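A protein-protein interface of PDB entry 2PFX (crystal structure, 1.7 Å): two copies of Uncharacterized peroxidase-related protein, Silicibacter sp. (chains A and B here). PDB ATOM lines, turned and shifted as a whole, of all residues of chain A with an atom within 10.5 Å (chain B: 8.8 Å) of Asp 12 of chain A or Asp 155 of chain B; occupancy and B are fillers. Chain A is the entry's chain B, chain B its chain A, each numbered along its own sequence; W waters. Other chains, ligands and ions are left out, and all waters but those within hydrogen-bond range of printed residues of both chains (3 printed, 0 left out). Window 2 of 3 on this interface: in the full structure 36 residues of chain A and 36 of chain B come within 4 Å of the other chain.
Printed residues of chain B within 4 Å of Asp 12 of chain A: Asp 155 (2.7 Å).
Asp 155 of chain B touches just these residues of chain A: Leu 11 and Asp 12.
No residue of chain A comes within 4 Å of Asn 154 of chain B.
No residue of chain A comes within 4 Å of Ile 158 of chain B.
Printed residues of chain A within 4 Å of Trp 159 of chain B: Leu 11, Leu 13, Ala 43, Phe 46, Val 174 and Thr 178.
Printed residues of chain B within 4 Å of Thr 178 of chain A: Arg 145 and Trp 159.
Printed residues of chain B within 4 Å of Phe 46 of chain A: Arg 156 (3.5 Å) and Trp 159 (3.7 Å).
Arg 149 of chain B touches none of the printed residues of chain A.
The nearest printed residue of chain A that does not touch Trp 159 of chain B is Thr 9 of chain A (4.4 Å).
NH2 of Arg 145 of chain B is in salt-bridge range of OE1 of Glu 142 of chain B (2.7 Å).
NH1 of Arg 149 of chain B lies within salt-bridge range of OD1 of Asp 155 of chain B, at 3.3 Å.
The side-chain carboxylate of Asp 160 of chain B lies within salt-bridge range of the guanidinium group of Arg 156 of chain B, 3.0 Å away.
The backbone carbonyl oxygen (O) of Leu 11 of chain A is in hydrogen-bond range of the side-chain amino group (NZ) of Lys 6 of chain A, 3.4 Å away.
The side-chain hydroxyl of Thr 9 of chain A lies within hydrogen-bond range of the backbone NH of Leu 11 of chain A (2.9 Å).
O of Val 174 of chain A is in hydrogen-bond range of OG1 of Thr 178 of chain A, 2.7 Å away.
Ala 10 of chain A touches Arg 145 of chain B (CB to NH2, 3.5 Å).
CD1 of Leu 11 of chain A touches N of Trp 159 of chain B, at 3.9 Å.
Leu 13 of chain A touches Arg 156 of chain B (CD2 to CA, 3.999 Å).
Trp 159 of chain B touches Leu 13 of chain A.
Trp 159 of chain B touches Ala 43 of chain A.
CE2 of Phe 46 of chain A touches CD of Arg 156 of chain B, 3.5 Å away.
Phe 46 of chain A touches Trp 159 of chain B (CE1 to NE1, 3.7 Å).
Ala 162 of chain B touches Val 174 of chain A (O to CG2, 3.8 Å).
Asn 163 of chain B touches Val 174 of chain A (ND2 to CG1, 3.9 Å).
Ala 179 of chain A touches Arg 145 of chain B (CB to NH2, 3.95 Å).
NH1 of Arg 145 of chain B lies within hydrogen-bond range of O of Ala 177 of chain A (3.0 Å).
OD2 of Asp 155 of chain B is in hydrogen-bond range of N of Asp 12 of chain A, at 2.7 Å.
Water W1 bridges the side-chain carboxylate of Asp 160 of chain B and the side-chain amino group of Lys 50 of chain A.
Water W2 lies within hydrogen-bond range of OE1 of Glu 142 of chain B, O of Ala 10 of chain A, NE of Arg 145 of chain B and NH1 of Arg 149 of chain B.
Water W3 lies within hydrogen-bond range of the side-chain amino group (NZ) of Lys 50 of chain A (3.3 Å) and the guanidinium group (NH2) of Arg 156 of chain B (3.4 Å).
Hydrophobic or aromatic side chains of chain B within 4 Å of the printed part of chain A: Trp 159.
Of the 19 printed residues of chain A, 11 touch a printed residue of chain B.
No position is printed for both chains.
Of the 18 pairs that touch across the chains among the printed residues, none has its exchanged pair printed and touching as well.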
ATOM      1  N   LYS A   6       6.389 -34.491 -14.065  1.00  0.00           N
ATOM      2  CA  LYS A   6       6.491 -34.168 -15.464  1.00  0.00           C
ATOM      3  C   LYS A   6       7.980 -34.174 -15.861  1.00  0.00           C
ATOM      4  O   LYS A   6       8.843 -33.839 -15.051  1.00  0.00           O
ATOM      5  CB  LYS A   6       5.847 -32.824 -15.812  1.00  0.00           C
ATOM      6  CG  LYS A   6       4.935 -32.777 -17.012  1.00  0.00           C
ATOM      7  CD  LYS A   6       5.585 -32.520 -18.350  1.00  0.00           C
ATOM      8  CE  LYS A   6       6.168 -31.121 -18.485  1.00  0.00           C
ATOM      9  NZ  LYS A   6       7.510 -31.182 -19.145  1.00  0.00           N
ATOM     10  N   GLU A   7       8.166 -34.573 -17.113  1.00  0.00           N
ATOM     11  CA  GLU A   7       9.432 -34.580 -17.822  1.00  0.00           C
ATOM     12  C   GLU A   7       9.315 -33.786 -19.100  1.00  0.00           C
ATOM     13  O   GLU A   7       8.256 -33.704 -19.714  1.00  0.00           O
ATOM     14  CB  GLU A   7       9.863 -36.024 -18.121  1.00  0.00           C
ATOM     15  CG  GLU A   7      10.095 -36.818 -16.845  1.00  0.00           C
ATOM     16  CD  GLU A   7      10.326 -38.301 -17.084  1.00  0.00           C
ATOM     17  OE1 GLU A   7      11.207 -38.630 -17.907  1.00  0.00           O
ATOM     18  OE2 GLU A   7       9.630 -39.130 -16.456  1.00  0.00           O
ATOM     19  N   PRO A   8      10.404 -33.172 -19.529  1.00  0.00           N
ATOM     20  CA  PRO A   8      11.655 -33.175 -18.787  1.00  0.00           C
ATOM     21  C   PRO A   8      11.712 -32.205 -17.611  1.00  0.00           C
ATOM     22  O   PRO A   8      12.599 -32.373 -16.782  1.00  0.00           O
ATOM     23  CB  PRO A   8      12.645 -32.702 -19.863  1.00  0.00           C
ATOM     24  CG  PRO A   8      11.831 -31.848 -20.779  1.00  0.00           C
ATOM     25  CD  PRO A   8      10.460 -32.446 -20.806  1.00  0.00           C
ATOM     26  N   THR A   9      10.843 -31.213 -17.535  1.00  0.00           N
ATOM     27  CA  THR A   9      10.706 -30.291 -16.428  1.00  0.00           C
ATOM     28  C   THR A   9       9.225 -30.102 -16.108  1.00  0.00           C
ATOM     29  O   THR A   9       8.358 -30.604 -16.828  1.00  0.00           O
ATOM     30  CB  THR A   9      11.279 -28.886 -16.668  1.00  0.00           C
ATOM     31  OG1 THR A   9      10.370 -28.115 -17.469  1.00  0.00           O
ATOM     32  CG2 THR A   9      12.614 -28.966 -17.399  1.00  0.00           C
ATOM     33  N   ALA A  10       8.948 -29.362 -15.050  1.00  0.00           N
ATOM     34  CA  ALA A  10       7.532 -29.106 -14.718  1.00  0.00           C
ATOM     35  C   ALA A  10       6.990 -27.899 -15.473  1.00  0.00           C
ATOM     36  O   ALA A  10       5.896 -27.393 -15.209  1.00  0.00           O
ATOM     37  CB  ALA A  10       7.354 -28.952 -13.215  1.00  0.00           C
ATOM     38  N   LEU A  11       7.735 -27.373 -16.425  1.00  0.00           N
ATOM     39  CA  LEU A  11       7.287 -26.267 -17.261  1.00  0.00           C
ATOM     40  C   LEU A  11       6.685 -26.789 -18.556  1.00  0.00           C
ATOM     41  O   LEU A  11       7.122 -27.793 -19.095  1.00  0.00           O
ATOM     42  CB  LEU A  11       8.430 -25.312 -17.597  1.00  0.00           C
ATOM     43  CG  LEU A  11       9.080 -24.656 -16.371  1.00  0.00           C
ATOM     44  CD1 LEU A  11      10.135 -23.636 -16.831  1.00  0.00           C
ATOM     45  CD2 LEU A  11       8.071 -23.990 -15.461  1.00  0.00           C
ATOM     46  N   ASP A  12       5.673 -26.072 -19.032  1.00  0.00           N
ATOM     47  CA  ASP A  12       5.106 -26.491 -20.331  1.00  0.00           C
ATOM     48  C   ASP A  12       5.870 -25.753 -21.415  1.00  0.00           C
ATOM     49  O   ASP A  12       5.592 -24.620 -21.818  1.00  0.00           O
ATOM     50  CB  ASP A  12       3.611 -26.224 -20.303  1.00  0.00           C
ATOM     51  CG  ASP A  12       2.927 -26.301 -21.650  1.00  0.00           C
ATOM     52  OD1 ASP A  12       3.550 -26.732 -22.638  1.00  0.00           O
ATOM     53  OD2 ASP A  12       1.744 -25.911 -21.711  1.00  0.00           O
ATOM     54  N   LEU A  13       6.908 -26.402 -21.907  1.00  0.00           N
ATOM     55  CA  LEU A  13       7.864 -25.901 -22.877  1.00  0.00           C
ATOM     56  C   LEU A  13       8.013 -26.931 -23.997  1.00  0.00           C
ATOM     57  O   LEU A  13       9.063 -27.549 -24.162  1.00  0.00           O
ATOM     58  CB  LEU A  13       9.209 -25.704 -22.196  1.00  0.00           C
ATOM     59  CG  LEU A  13       9.591 -24.428 -21.475  1.00  0.00           C
ATOM     60  CD1 LEU A  13      10.911 -24.635 -20.730  1.00  0.00           C
ATOM     61  CD2 LEU A  13       9.701 -23.275 -22.451  1.00  0.00           C
ATOM     62  N   PRO A  14       6.952 -27.148 -24.761  1.00  0.00           N
ATOM     63  CA  PRO A  14       6.931 -28.128 -25.848  1.00  0.00           C
ATOM     64  C   PRO A  14       8.097 -27.939 -26.821  1.00  0.00           C
ATOM     65  O   PRO A  14       8.526 -26.811 -27.059  1.00  0.00           O
ATOM     66  CB  PRO A  14       5.605 -27.845 -26.551  1.00  0.00           C
ATOM     67  CG  PRO A  14       5.083 -26.556 -26.010  1.00  0.00           C
ATOM     68  CD  PRO A  14       5.649 -26.445 -24.630  1.00  0.00           C
ATOM     69  N   MET A  15       8.583 -29.040 -27.394  1.00  0.00           N
ATOM     70  CA  MET A  15       9.767 -29.100 -28.225  1.00  0.00           C
ATOM     71  C   MET A  15       9.690 -28.588 -29.654  1.00  0.00           C
ATOM     72  O   MET A  15      10.550 -27.762 -30.028  1.00  0.00           O
ATOM     73  CB  MET A  15      10.271 -30.568 -28.292  1.00  0.00           C
ATOM     74  CG  MET A  15      11.748 -30.679 -27.973  1.00  0.00           C
ATOM     75  SD  MET A  15      12.312 -32.316 -27.182  1.00  0.00           S
ATOM     76  CE  MET A  15      12.784 -33.243 -28.736  1.00  0.00           C
ATOM     77  N   ALA A  16       8.785 -28.999 -30.502  1.00  0.00           N
ATOM     78  CA  ALA A  16       7.760 -30.003 -30.418  1.00  0.00           C
ATOM     79  C   ALA A  16       8.051 -31.086 -31.474  1.00  0.00           C
ATOM     80  O   ALA A  16       9.029 -30.931 -32.208  1.00  0.00           O
ATOM     81  CB  ALA A  16       6.372 -29.413 -30.602  1.00  0.00           C
ATOM     82  N   LYS A  42      16.453 -32.113 -23.835  1.00  0.00           N
ATOM     83  CA  LYS A  42      15.054 -31.955 -24.252  1.00  0.00           C
ATOM     84  C   LYS A  42      14.446 -30.680 -23.701  1.00  0.00           C
ATOM     85  O   LYS A  42      13.570 -30.074 -24.324  1.00  0.00           O
ATOM     86  CB  LYS A  42      14.234 -33.171 -23.816  1.00  0.00           C
ATOM     87  CG  LYS A  42      14.652 -34.456 -24.517  1.00  0.00           C
ATOM     88  CD  LYS A  42      13.885 -35.640 -23.948  1.00  0.00           C
ATOM     89  CE  LYS A  42      14.258 -36.943 -24.637  1.00  0.00           C
ATOM     90  NZ  LYS A  42      14.727 -38.003 -23.691  1.00  0.00           N
ATOM     91  N   ALA A  43      14.911 -30.238 -22.520  1.00  0.00           N
ATOM     92  CA  ALA A  43      14.383 -28.999 -21.946  1.00  0.00           C
ATOM     93  C   ALA A  43      14.823 -27.781 -22.732  1.00  0.00           C
ATOM     94  O   ALA A  43      14.054 -26.826 -22.801  1.00  0.00           O
ATOM     95  CB  ALA A  43      14.800 -28.834 -20.498  1.00  0.00           C
ATOM     96  N   PHE A  46      13.378 -26.761 -27.013  1.00  0.00           N
ATOM     97  CA  PHE A  46      12.293 -25.980 -27.613  1.00  0.00           C
ATOM     98  C   PHE A  46      12.822 -24.843 -28.476  1.00  0.00           C
ATOM     99  O   PHE A  46      12.110 -24.221 -29.271  1.00  0.00           O
ATOM    100  CB  PHE A  46      11.350 -25.411 -26.536  1.00  0.00           C
ATOM    101  CG  PHE A  46      11.981 -24.288 -25.737  1.00  0.00           C
ATOM    102  CD1 PHE A  46      12.834 -24.599 -24.690  1.00  0.00           C
ATOM    103  CD2 PHE A  46      11.730 -22.959 -26.010  1.00  0.00           C
ATOM    104  CE1 PHE A  46      13.420 -23.589 -23.955  1.00  0.00           C
ATOM    105  CE2 PHE A  46      12.329 -21.932 -25.292  1.00  0.00           C
ATOM    106  CZ  PHE A  46      13.179 -22.263 -24.260  1.00  0.00           C
ATOM    107  N   LYS A  50      19.184 -21.831 -28.077  1.00  0.00           N
ATOM    108  CA  LYS A  50      19.442 -21.993 -26.655  1.00  0.00           C
ATOM    109  C   LYS A  50      20.119 -23.335 -26.436  1.00  0.00           C
ATOM    110  O   LYS A  50      21.063 -23.469 -25.657  1.00  0.00           O
ATOM    111  CB  LYS A  50      18.146 -21.918 -25.840  1.00  0.00           C
ATOM    112  CG  LYS A  50      17.407 -20.602 -26.025  1.00  0.00           C
ATOM    113  CD  LYS A  50      16.230 -20.397 -25.087  1.00  0.00           C
ATOM    114  CE  LYS A  50      15.711 -18.972 -25.037  1.00  0.00           C
ATOM    115  NZ  LYS A  50      16.735 -17.956 -24.637  1.00  0.00           N
ATOM    116  N   VAL A 174      19.059 -23.969 -12.482  1.00  0.00           N
ATOM    117  CA  VAL A 174      18.056 -24.147 -13.529  1.00  0.00           C
ATOM    118  C   VAL A 174      17.278 -25.435 -13.308  1.00  0.00           C
ATOM    119  O   VAL A 174      16.057 -25.561 -13.445  1.00  0.00           O
ATOM    120  CB  VAL A 174      18.733 -24.176 -14.906  1.00  0.00           C
ATOM    121  CG1 VAL A 174      17.709 -24.482 -16.002  1.00  0.00           C
ATOM    122  CG2 VAL A 174      19.446 -22.866 -15.216  1.00  0.00           C
ATOM    123  N   ALA A 177      15.164 -25.125 -10.063  1.00  0.00           N
ATOM    124  CA  ALA A 177      14.055 -24.174 -10.135  1.00  0.00           C
ATOM    125  C   ALA A 177      12.952 -24.621 -11.066  1.00  0.00           C
ATOM    126  O   ALA A 177      11.810 -24.163 -10.908  1.00  0.00           O
ATOM    127  CB  ALA A 177      14.563 -22.817 -10.595  1.00  0.00           C
ATOM    128  N   THR A 178      13.254 -25.469 -12.030  1.00  0.00           N
ATOM    129  CA  THR A 178      12.257 -25.935 -12.984  1.00  0.00           C
ATOM    130  C   THR A 178      11.778 -27.359 -12.743  1.00  0.00           C
ATOM    131  O   THR A 178      11.012 -27.874 -13.570  1.00  0.00           O
ATOM    132  CB  THR A 178      12.778 -25.817 -14.431  1.00  0.00           C
ATOM    133  OG1 THR A 178      13.874 -26.709 -14.613  1.00  0.00           O
ATOM    134  CG2 THR A 178      13.266 -24.402 -14.742  1.00  0.00           C
ATOM    135  N   ALA A 179      12.214 -28.009 -11.674  1.00  0.00           N
ATOM    136  CA  ALA A 179      11.895 -29.391 -11.351  1.00  0.00           C
ATOM    137  C   ALA A 179      12.236 -30.347 -12.499  1.00  0.00           C
ATOM    138  O   ALA A 179      11.469 -31.230 -12.895  1.00  0.00           O
ATOM    139  CB  ALA A 179      10.451 -29.573 -10.943  1.00  0.00           C
ATOM    140  N   GLU B 142       6.538 -25.788  -6.714  1.00  0.00           N
ATOM    141  CA  GLU B 142       5.521 -25.404  -7.690  1.00  0.00           C
ATOM    142  C   GLU B 142       4.836 -24.111  -7.287  1.00  0.00           C
ATOM    143  O   GLU B 142       4.531 -23.269  -8.119  1.00  0.00           O
ATOM    144  CB  GLU B 142       4.542 -26.568  -7.802  1.00  0.00           C
ATOM    145  CG  GLU B 142       3.462 -26.312  -8.826  1.00  0.00           C
ATOM    146  CD  GLU B 142       3.942 -26.151 -10.241  1.00  0.00           C
ATOM    147  OE1 GLU B 142       4.902 -26.801 -10.677  1.00  0.00           O
ATOM    148  OE2 GLU B 142       3.327 -25.353 -10.985  1.00  0.00           O
ATOM    149  N   ARG B 145       6.705 -21.104  -8.535  1.00  0.00           N
ATOM    150  CA  ARG B 145       6.475 -20.865  -9.954  1.00  0.00           C
ATOM    151  C   ARG B 145       5.081 -20.275 -10.182  1.00  0.00           C
ATOM    152  O   ARG B 145       4.878 -19.463 -11.083  1.00  0.00           O
ATOM    153  CB  ARG B 145       6.687 -22.159 -10.737  1.00  0.00           C
ATOM    154  CG  ARG B 145       8.160 -22.575 -10.744  1.00  0.00           C
ATOM    155  CD  ARG B 145       8.434 -23.692 -11.730  1.00  0.00           C
ATOM    156  NE  ARG B 145       7.769 -24.942 -11.384  1.00  0.00           N
ATOM    157  CZ  ARG B 145       8.266 -25.850 -10.561  1.00  0.00           C
ATOM    158  NH1 ARG B 145       9.439 -25.715  -9.963  1.00  0.00           N
ATOM    159  NH2 ARG B 145       7.569 -26.947 -10.308  1.00  0.00           N
ATOM    160  N   GLU B 146       4.111 -20.659  -9.361  1.00  0.00           N
ATOM    161  CA  GLU B 146       2.761 -20.119  -9.576  1.00  0.00           C
ATOM    162  C   GLU B 146       2.701 -18.655  -9.192  1.00  0.00           C
ATOM    163  O   GLU B 146       1.908 -17.875  -9.751  1.00  0.00           O
ATOM    164  CB  GLU B 146       1.728 -20.929  -8.791  1.00  0.00           C
ATOM    165  CG  GLU B 146       0.282 -20.583  -9.179  1.00  0.00           C
ATOM    166  CD  GLU B 146      -0.024 -20.818 -10.639  1.00  0.00           C
ATOM    167  OE1 GLU B 146       0.407 -21.848 -11.225  1.00  0.00           O
ATOM    168  OE2 GLU B 146      -0.711 -19.946 -11.227  1.00  0.00           O
ATOM    169  N   LEU B 148       4.939 -16.501  -9.861  1.00  0.00           N
ATOM    170  CA  LEU B 148       5.337 -15.823 -11.091  1.00  0.00           C
ATOM    171  C   LEU B 148       4.206 -15.767 -12.108  1.00  0.00           C
ATOM    172  O   LEU B 148       3.979 -14.742 -12.756  1.00  0.00           O
ATOM    173  CB  LEU B 148       6.553 -16.519 -11.716  1.00  0.00           C
ATOM    174  CG  LEU B 148       7.781 -16.547 -10.804  1.00  0.00           C
ATOM    175  CD1 LEU B 148       8.879 -17.358 -11.485  1.00  0.00           C
ATOM    176  CD2 LEU B 148       8.241 -15.148 -10.453  1.00  0.00           C
ATOM    177  N   ARG B 149       3.503 -16.900 -12.271  1.00  0.00           N
ATOM    178  CA  ARG B 149       2.369 -16.886 -13.193  1.00  0.00           C
ATOM    179  C   ARG B 149       1.255 -15.941 -12.735  1.00  0.00           C
ATOM    180  O   ARG B 149       0.578 -15.352 -13.583  1.00  0.00           O
ATOM    181  CB  ARG B 149       1.772 -18.277 -13.360  1.00  0.00           C
ATOM    182  CG  ARG B 149       2.772 -19.279 -13.934  1.00  0.00           C
ATOM    183  CD  ARG B 149       2.151 -20.588 -14.384  1.00  0.00           C
ATOM    184  NE  ARG B 149       2.016 -21.545 -13.303  1.00  0.00           N
ATOM    185  CZ  ARG B 149       2.760 -22.569 -12.963  1.00  0.00           C
ATOM    186  NH1 ARG B 149       3.841 -22.902 -13.641  1.00  0.00           N
ATOM    187  NH2 ARG B 149       2.362 -23.250 -11.899  1.00  0.00           N
ATOM    188  N   GLY B 152       1.870 -12.589 -14.264  1.00  0.00           N
ATOM    189  CA  GLY B 152       1.851 -12.429 -15.688  1.00  0.00           C
ATOM    190  C   GLY B 152       2.963 -13.121 -16.435  1.00  0.00           C
ATOM    191  O   GLY B 152       2.974 -13.009 -17.667  1.00  0.00           O
ATOM    192  N   PHE B 153       3.860 -13.830 -15.736  1.00  0.00           N
ATOM    193  CA  PHE B 153       4.877 -14.607 -16.442  1.00  0.00           C
ATOM    194  C   PHE B 153       4.340 -15.954 -16.908  1.00  0.00           C
ATOM    195  O   PHE B 153       3.709 -16.683 -16.141  1.00  0.00           O
ATOM    196  CB  PHE B 153       6.094 -14.852 -15.544  1.00  0.00           C
ATOM    197  CG  PHE B 153       6.785 -13.564 -15.138  1.00  0.00           C
ATOM    198  CD1 PHE B 153       7.504 -12.841 -16.081  1.00  0.00           C
ATOM    199  CD2 PHE B 153       6.709 -13.091 -13.848  1.00  0.00           C
ATOM    200  CE1 PHE B 153       8.159 -11.670 -15.723  1.00  0.00           C
ATOM    201  CE2 PHE B 153       7.377 -11.943 -13.471  1.00  0.00           C
ATOM    202  CZ  PHE B 153       8.108 -11.239 -14.411  1.00  0.00           C
ATOM    203  N   ASN B 154       4.602 -16.297 -18.165  1.00  0.00           N
ATOM    204  CA  ASN B 154       4.274 -17.630 -18.622  1.00  0.00           C
ATOM    205  C   ASN B 154       5.474 -18.568 -18.416  1.00  0.00           C
ATOM    206  O   ASN B 154       6.495 -18.203 -17.842  1.00  0.00           O
ATOM    207  CB  ASN B 154       3.813 -17.576 -20.066  1.00  0.00           C
ATOM    208  CG  ASN B 154       4.872 -17.235 -21.079  1.00  0.00           C
ATOM    209  OD1 ASN B 154       6.056 -17.178 -20.759  1.00  0.00           O
ATOM    210  ND2 ASN B 154       4.442 -17.003 -22.316  1.00  0.00           N
ATOM    211  N   ASP B 155       5.361 -19.806 -18.876  1.00  0.00           N
ATOM    212  CA  ASP B 155       6.376 -20.795 -18.505  1.00  0.00           C
ATOM    213  C   ASP B 155       7.672 -20.530 -19.262  1.00  0.00           C
ATOM    214  O   ASP B 155       8.743 -20.823 -18.730  1.00  0.00           O
ATOM    215  CB  ASP B 155       5.895 -22.209 -18.763  1.00  0.00           C
ATOM    216  CG  ASP B 155       5.044 -22.768 -17.650  1.00  0.00           C
ATOM    217  OD1 ASP B 155       4.697 -22.020 -16.710  1.00  0.00           O
ATOM    218  OD2 ASP B 155       4.720 -23.971 -17.719  1.00  0.00           O
ATOM    219  N   ARG B 156       7.558 -19.970 -20.456  1.00  0.00           N
ATOM    220  CA  ARG B 156       8.776 -19.601 -21.170  1.00  0.00           C
ATOM    221  C   ARG B 156       9.484 -18.504 -20.395  1.00  0.00           C
ATOM    222  O   ARG B 156      10.697 -18.466 -20.297  1.00  0.00           O
ATOM    223  CB  ARG B 156       8.415 -19.183 -22.588  1.00  0.00           C
ATOM    224  CG  ARG B 156       9.516 -18.532 -23.375  1.00  0.00           C
ATOM    225  CD  ARG B 156      10.815 -19.322 -23.598  1.00  0.00           C
ATOM    226  NE  ARG B 156      11.824 -18.246 -23.747  1.00  0.00           N
ATOM    227  CZ  ARG B 156      12.103 -17.581 -24.858  1.00  0.00           C
ATOM    228  NH1 ARG B 156      11.523 -17.849 -26.015  1.00  0.00           N
ATOM    229  NH2 ARG B 156      13.014 -16.618 -24.850  1.00  0.00           N
ATOM    230  N   ASP B 157       8.723 -17.578 -19.827  1.00  0.00           N
ATOM    231  CA  ASP B 157       9.309 -16.492 -19.069  1.00  0.00           C
ATOM    232  C   ASP B 157      10.047 -17.028 -17.835  1.00  0.00           C
ATOM    233  O   ASP B 157      11.127 -16.551 -17.495  1.00  0.00           O
ATOM    234  CB  ASP B 157       8.227 -15.524 -18.600  1.00  0.00           C
ATOM    235  CG  ASP B 157       7.545 -14.789 -19.723  1.00  0.00           C
ATOM    236  OD1 ASP B 157       8.073 -14.793 -20.852  1.00  0.00           O
ATOM    237  OD2 ASP B 157       6.472 -14.208 -19.456  1.00  0.00           O
ATOM    238  N   ILE B 158       9.428 -17.973 -17.149  1.00  0.00           N
ATOM    239  CA  ILE B 158      10.033 -18.578 -15.958  1.00  0.00           C
ATOM    240  C   ILE B 158      11.344 -19.248 -16.335  1.00  0.00           C
ATOM    241  O   ILE B 158      12.373 -19.126 -15.663  1.00  0.00           O
ATOM    242  CB  ILE B 158       9.049 -19.566 -15.303  1.00  0.00           C
ATOM    243  CG1 ILE B 158       7.725 -18.908 -14.926  1.00  0.00           C
ATOM    244  CG2 ILE B 158       9.699 -20.220 -14.098  1.00  0.00           C
ATOM    245  CD1 ILE B 158       6.767 -19.796 -14.155  1.00  0.00           C
ATOM    246  N   TRP B 159      11.345 -19.957 -17.461  1.00  0.00           N
ATOM    247  CA  TRP B 159      12.574 -20.564 -17.969  1.00  0.00           C
ATOM    248  C   TRP B 159      13.680 -19.529 -18.181  1.00  0.00           C
ATOM    249  O   TRP B 159      14.854 -19.703 -17.833  1.00  0.00           O
ATOM    250  CB  TRP B 159      12.315 -21.274 -19.294  1.00  0.00           C
ATOM    251  CG  TRP B 159      13.548 -21.864 -19.902  1.00  0.00           C
ATOM    252  CD1 TRP B 159      14.340 -21.348 -20.879  1.00  0.00           C
ATOM    253  CD2 TRP B 159      14.142 -23.130 -19.535  1.00  0.00           C
ATOM    254  NE1 TRP B 159      15.386 -22.204 -21.159  1.00  0.00           N
ATOM    255  CE2 TRP B 159      15.276 -23.304 -20.339  1.00  0.00           C
ATOM    256  CE3 TRP B 159      13.806 -24.116 -18.610  1.00  0.00           C
ATOM    257  CZ2 TRP B 159      16.087 -24.431 -20.244  1.00  0.00           C
ATOM    258  CZ3 TRP B 159      14.598 -25.247 -18.503  1.00  0.00           C
ATOM    259  CH2 TRP B 159      15.728 -25.383 -19.327  1.00  0.00           C
ATOM    260  N   ASP B 160      13.303 -18.404 -18.794  1.00  0.00           N
ATOM    261  CA  ASP B 160      14.244 -17.307 -18.968  1.00  0.00           C
ATOM    262  C   ASP B 160      14.717 -16.736 -17.646  1.00  0.00           C
ATOM    263  O   ASP B 160      15.893 -16.412 -17.494  1.00  0.00           O
ATOM    264  CB  ASP B 160      13.588 -16.214 -19.807  1.00  0.00           C
ATOM    265  CG  ASP B 160      13.400 -16.560 -21.269  1.00  0.00           C
ATOM    266  OD1 ASP B 160      13.842 -17.677 -21.634  1.00  0.00           O
ATOM    267  OD2 ASP B 160      12.814 -15.744 -22.036  1.00  0.00           O
ATOM    268  N   ILE B 161      13.823 -16.575 -16.665  1.00  0.00           N
ATOM    269  CA  ILE B 161      14.289 -16.031 -15.388  1.00  0.00           C
ATOM    270  C   ILE B 161      15.291 -16.967 -14.740  1.00  0.00           C
ATOM    271  O   ILE B 161      16.342 -16.597 -14.192  1.00  0.00           O
ATOM    272  CB  ILE B 161      13.096 -15.750 -14.454  1.00  0.00           C
ATOM    273  CG1 ILE B 161      12.196 -14.594 -14.915  1.00  0.00           C
ATOM    274  CG2 ILE B 161      13.583 -15.469 -13.044  1.00  0.00           C
ATOM    275  CD1 ILE B 161      10.803 -14.683 -14.326  1.00  0.00           C
ATOM    276  N   ALA B 162      14.975 -18.263 -14.809  1.00  0.00           N
ATOM    277  CA  ALA B 162      15.854 -19.283 -14.258  1.00  0.00           C
ATOM    278  C   ALA B 162      17.205 -19.278 -14.967  1.00  0.00           C
ATOM    279  O   ALA B 162      18.243 -19.419 -14.315  1.00  0.00           O
ATOM    280  CB  ALA B 162      15.208 -20.652 -14.353  1.00  0.00           C
ATOM    281  N   ASN B 163      17.221 -19.121 -16.281  1.00  0.00           N
ATOM    282  CA  ASN B 163      18.527 -19.223 -16.957  1.00  0.00           C
ATOM    283  C   ASN B 163      19.368 -17.986 -16.723  1.00  0.00           C
ATOM    284  O   ASN B 163      20.582 -18.099 -16.513  1.00  0.00           O
ATOM    285  CB  ASN B 163      18.323 -19.519 -18.441  1.00  0.00           C
ATOM    286  CG  ASN B 163      18.214 -21.017 -18.659  1.00  0.00           C
ATOM    287  OD1 ASN B 163      19.196 -21.664 -19.025  1.00  0.00           O
ATOM    288  ND2 ASN B 163      17.027 -21.558 -18.419  1.00  0.00           N
HETATM  289  O   HOH W   1      16.462 -18.189 -21.657  1.00  0.00           O
HETATM  290  O   HOH W   2       5.570 -25.707 -13.040  1.00  0.00           O
HETATM  291  O   HOH W   3      15.494 -16.144 -27.120  1.00  0.00           O
